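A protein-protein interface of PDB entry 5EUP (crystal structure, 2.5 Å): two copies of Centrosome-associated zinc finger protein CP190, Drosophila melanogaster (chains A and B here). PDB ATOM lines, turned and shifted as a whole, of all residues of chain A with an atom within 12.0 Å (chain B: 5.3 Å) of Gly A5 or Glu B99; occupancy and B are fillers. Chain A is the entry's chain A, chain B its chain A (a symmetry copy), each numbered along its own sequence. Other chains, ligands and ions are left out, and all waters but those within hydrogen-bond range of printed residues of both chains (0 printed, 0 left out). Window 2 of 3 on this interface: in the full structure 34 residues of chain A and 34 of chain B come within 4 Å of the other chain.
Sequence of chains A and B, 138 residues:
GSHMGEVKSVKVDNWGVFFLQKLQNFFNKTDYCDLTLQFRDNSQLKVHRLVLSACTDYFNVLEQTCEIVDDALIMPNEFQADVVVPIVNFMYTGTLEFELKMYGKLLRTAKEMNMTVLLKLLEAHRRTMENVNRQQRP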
ATOM      1  N   GLY A   5       2.244 -36.786  -6.507  1.00  0.00           N
ATOM      2  CA  GLY A   5       3.271 -36.085  -7.254  1.00  0.00           C
ATOM      3  C   GLY A   5       3.514 -34.682  -6.735  1.00  0.00           C
ATOM      4  O   GLY A   5       2.598 -34.025  -6.237  1.00  0.00           O
ATOM      5  N   GLU A   6       4.755 -34.220  -6.851  1.00  0.00           N
ATOM      6  CA  GLU A   6       5.122 -32.885  -6.392  1.00  0.00           C
ATOM      7  C   GLU A   6       4.792 -31.831  -7.445  1.00  0.00           C
ATOM      8  O   GLU A   6       5.001 -32.046  -8.639  1.00  0.00           O
ATOM      9  CB  GLU A   6       6.609 -32.833  -6.026  1.00  0.00           C
ATOM     10  CG  GLU A   6       7.138 -31.444  -5.683  1.00  0.00           C
ATOM     11  CD  GLU A   6       6.437 -30.820  -4.493  1.00  0.00           C
ATOM     12  OE1 GLU A   6       5.979 -31.569  -3.603  1.00  0.00           O
ATOM     13  OE2 GLU A   6       6.346 -29.574  -4.451  1.00  0.00           O
ATOM     14  N   VAL A   7       4.271 -30.696  -6.992  1.00  0.00           N
ATOM     15  CA  VAL A   7       3.922 -29.605  -7.892  1.00  0.00           C
ATOM     16  C   VAL A   7       5.181 -28.925  -8.422  1.00  0.00           C
ATOM     17  O   VAL A   7       6.015 -28.457  -7.648  1.00  0.00           O
ATOM     18  CB  VAL A   7       3.039 -28.560  -7.190  1.00  0.00           C
ATOM     19  CG1 VAL A   7       2.484 -27.573  -8.201  1.00  0.00           C
ATOM     20  CG2 VAL A   7       1.909 -29.244  -6.445  1.00  0.00           C
ATOM     21  N   LYS A   8       5.312 -28.875  -9.744  1.00  0.00           N
ATOM     22  CA  LYS A   8       6.489 -28.292 -10.378  1.00  0.00           C
ATOM     23  C   LYS A   8       6.236 -26.841 -10.771  1.00  0.00           C
ATOM     24  O   LYS A   8       5.095 -26.379 -10.757  1.00  0.00           O
ATOM     25  CB  LYS A   8       6.895 -29.113 -11.602  1.00  0.00           C
ATOM     26  CG  LYS A   8       7.052 -30.599 -11.320  1.00  0.00           C
ATOM     27  CD  LYS A   8       8.053 -30.846 -10.200  1.00  0.00           C
ATOM     28  CE  LYS A   8       8.210 -32.332  -9.911  1.00  0.00           C
ATOM     29  NZ  LYS A   8       8.757 -33.071 -11.082  1.00  0.00           N
ATOM     30  N   SER A   9       7.299 -26.123 -11.120  1.00  0.00           N
ATOM     31  CA  SER A   9       7.171 -24.709 -11.459  1.00  0.00           C
ATOM     32  C   SER A   9       8.203 -24.236 -12.479  1.00  0.00           C
ATOM     33  O   SER A   9       9.409 -24.387 -12.282  1.00  0.00           O
ATOM     34  CB  SER A   9       7.256 -23.847 -10.196  1.00  0.00           C
ATOM     35  OG  SER A   9       8.531 -23.961  -9.589  1.00  0.00           O
ATOM     36  N   VAL A  10       7.711 -23.662 -13.572  1.00  0.00           N
ATOM     37  CA  VAL A  10       8.561 -23.007 -14.557  1.00  0.00           C
ATOM     38  C   VAL A  10       8.099 -21.563 -14.720  1.00  0.00           C
ATOM     39  O   VAL A  10       6.913 -21.266 -14.571  1.00  0.00           O
ATOM     40  CB  VAL A  10       8.520 -23.726 -15.918  1.00  0.00           C
ATOM     41  CG1 VAL A  10       9.227 -25.070 -15.831  1.00  0.00           C
ATOM     42  CG2 VAL A  10       7.085 -23.902 -16.389  1.00  0.00           C
ATOM     43  N   GLU B  97       2.603 -22.656 -11.868  1.00  0.00           N
ATOM     44  CA  GLU B  97       2.638 -23.691 -10.844  1.00  0.00           C
ATOM     45  C   GLU B  97       1.682 -24.815 -11.224  1.00  0.00           C
ATOM     46  O   GLU B  97       0.480 -24.586 -11.372  1.00  0.00           O
ATOM     47  CB  GLU B  97       2.248 -23.093  -9.492  1.00  0.00           C
ATOM     48  CG  GLU B  97       2.304 -24.059  -8.330  1.00  0.00           C
ATOM     49  CD  GLU B  97       1.881 -23.414  -7.026  1.00  0.00           C
ATOM     50  OE1 GLU B  97       2.637 -22.563  -6.510  1.00  0.00           O
ATOM     51  OE2 GLU B  97       0.790 -23.755  -6.523  1.00  0.00           O
ATOM     52  N   PHE B  98       2.209 -26.025 -11.387  1.00  0.00           N
ATOM     53  CA  PHE B  98       1.395 -27.140 -11.868  1.00  0.00           C
ATOM     54  C   PHE B  98       1.961 -28.520 -11.532  1.00  0.00           C
ATOM     55  O   PHE B  98       3.152 -28.671 -11.260  1.00  0.00           O
ATOM     56  CB  PHE B  98       1.199 -27.028 -13.382  1.00  0.00           C
ATOM     57  CG  PHE B  98       2.443 -27.311 -14.182  1.00  0.00           C
ATOM     58  CD1 PHE B  98       2.624 -28.543 -14.790  1.00  0.00           C
ATOM     59  CD2 PHE B  98       3.428 -26.348 -14.329  1.00  0.00           C
ATOM     60  CE1 PHE B  98       3.762 -28.811 -15.526  1.00  0.00           C
ATOM     61  CE2 PHE B  98       4.571 -26.611 -15.065  1.00  0.00           C
ATOM     62  CZ  PHE B  98       4.736 -27.845 -15.664  1.00  0.00           C
ATOM     63  N   GLU B  99       1.084 -29.520 -11.553  1.00  0.00           N
ATOM     64  CA  GLU B  99       1.486 -30.916 -11.437  1.00  0.00           C
ATOM     65  C   GLU B  99       1.786 -31.472 -12.823  1.00  0.00           C
ATOM     66  O   GLU B  99       1.168 -31.064 -13.806  1.00  0.00           O
ATOM     67  CB  GLU B  99       0.381 -31.743 -10.782  1.00  0.00           C
ATOM     68  CG  GLU B  99       0.387 -31.727  -9.263  1.00  0.00           C
ATOM     69  CD  GLU B  99       0.675 -33.096  -8.675  1.00  0.00           C
ATOM     70  OE1 GLU B  99       0.147 -33.401  -7.585  1.00  0.00           O
ATOM     71  OE2 GLU B  99       1.430 -33.866  -9.305  1.00  0.00           O
ATOM     72  N   LEU B 100       2.725 -32.411 -12.897  1.00  0.00           N
ATOM     73  CA  LEU B 100       3.138 -32.989 -14.175  1.00  0.00           C
ATOM     74  C   LEU B 100       1.995 -33.689 -14.907  1.00  0.00           C
ATOM     75  O   LEU B 100       1.994 -33.769 -16.135  1.00  0.00           O
ATOM     76  CB  LEU B 100       4.297 -33.967 -13.975  1.00  0.00           C
ATOM     77  CG  LEU B 100       5.636 -33.352 -13.566  1.00  0.00           C
ATOM     78  CD1 LEU B 100       6.694 -34.431 -13.422  1.00  0.00           C
ATOM     79  CD2 LEU B 100       6.066 -32.304 -14.580  1.00  0.00           C
ATOM     80  N   LYS B 101       1.025 -34.189 -14.150  1.00  0.00           N
ATOM     81  CA  LYS B 101      -0.113 -34.889 -14.737  1.00  0.00           C
ATOM     82  C   LYS B 101      -1.028 -33.922 -15.486  1.00  0.00           C
ATOM     83  O   LYS B 101      -1.839 -34.336 -16.317  1.00  0.00           O
ATOM     84  CB  LYS B 101      -0.897 -35.631 -13.653  1.00  0.00           C
ATOM     85  CG  LYS B 101      -1.902 -36.639 -14.186  1.00  0.00           C
ATOM     86  CD  LYS B 101      -2.600 -37.369 -13.052  1.00  0.00           C
ATOM     87  CE  LYS B 101      -3.581 -38.405 -13.579  1.00  0.00           C
ATOM     88  NZ  LYS B 101      -4.288 -39.114 -12.476  1.00  0.00           N
ATOM     89  N   MET B 102      -0.884 -32.633 -15.196  1.00  0.00           N
ATOM     90  CA  MET B 102      -1.712 -31.605 -15.814  1.00  0.00           C
ATOM     91  C   MET B 102      -1.046 -30.973 -17.036  1.00  0.00           C
ATOM     92  O   MET B 102      -1.608 -30.066 -17.650  1.00  0.00           O
ATOM     93  CB  MET B 102      -2.052 -30.514 -14.795  1.00  0.00           C
ATOM     94  CG  MET B 102      -3.007 -30.953 -13.698  1.00  0.00           C
ATOM     95  SD  MET B 102      -4.645 -31.341 -14.340  1.00  0.00           S
ATOM     96  CE  MET B 102      -5.044 -29.809 -15.176  1.00  0.00           C
ATOM     97  N   TYR B 103       0.143 -31.455 -17.387  1.00  0.00           N
ATOM     98  CA  TYR B 103       0.931 -30.852 -18.462  1.00  0.00           C
ATOM     99  C   TYR B 103       0.203 -30.806 -19.804  1.00  0.00           C
ATOM    100  O   TYR B 103       0.056 -29.741 -20.402  1.00  0.00           O
ATOM    101  CB  TYR B 103       2.271 -31.575 -18.628  1.00  0.00           C
ATOM    102  CG  TYR B 103       3.071 -31.088 -19.815  1.00  0.00           C
ATOM    103  CD1 TYR B 103       3.751 -29.878 -19.770  1.00  0.00           C
ATOM    104  CD2 TYR B 103       3.145 -31.838 -20.985  1.00  0.00           C
ATOM    105  CE1 TYR B 103       4.480 -29.427 -20.856  1.00  0.00           C
ATOM    106  CE2 TYR B 103       3.872 -31.395 -22.074  1.00  0.00           C
ATOM    107  CZ  TYR B 103       4.538 -30.190 -22.004  1.00  0.00           C
ATOM    108  OH  TYR B 103       5.263 -29.746 -23.085  1.00  0.00           O
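Printed residues of chain A that touch a printed residue of chain B: Gly A5, Val A7, Lys A8 and Val A10.
Of the 7 printed residues of chain B, 4 touch a printed residue of chain A.
Among the printed residues, no Asp or Glu carboxylate lies within 4 Å of a Lys or Arg side-chain nitrogen of the other chain.
Val A7 touches Glu B97 (CG1 to CG, 3.5 Å).
Val A7 touches Phe B98 (CG1 to O, 3.3 Å).
O of Lys A8 touches CA of Glu B97, at 3.6 Å.
NZ of Lys A8 touches CD1 of Leu B100, at 3.4 Å.
Phe B98 touches Val A10.
The backbone NH (N) of Lys A8 sits at hydrogen-bond distance from the backbone carbonyl oxygen (O) of Phe B98 (2.6 Å).
The backbone carbonyl oxygen (O) of Gly A5 lies close to the side-chain carboxylate (OE1) of Glu B99 (2.9 Å).
Of chain B, only Glu B99 comes within 4 Å of Gly A5.
Of the printed residues of chain B, Val A7 touches Glu B97 (3.5 Å) and Phe B98 (3.3 Å).
Printed residues of chain B within 4 Å of Lys A8: Glu B97 (3.6 Å), Phe B98 (2.6 Å) and Leu B100 (3.4 Å).
Printed residues of chain B within 4 Å of Val A10: Phe B98 (3.9 Å).
Of the printed residues of chain A, Glu B97 touches Val A7 and Lys A8.
Of chain A, only Val A7, Lys A8 and Val A10 come within 4 Å of Phe B98.
Leu B100 touches just one residue of chain A: Lys A8.
No residue of chain A comes within 4 Å of Met B102.
The nearest printed residue of chain A that does not touch Glu B97 is Ser A9 (4.7 Å).
No position is printed for both chains.
Of the 7 pairs that touch across the chains among the printed residues, none has its exchanged pair printed and touching as well.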
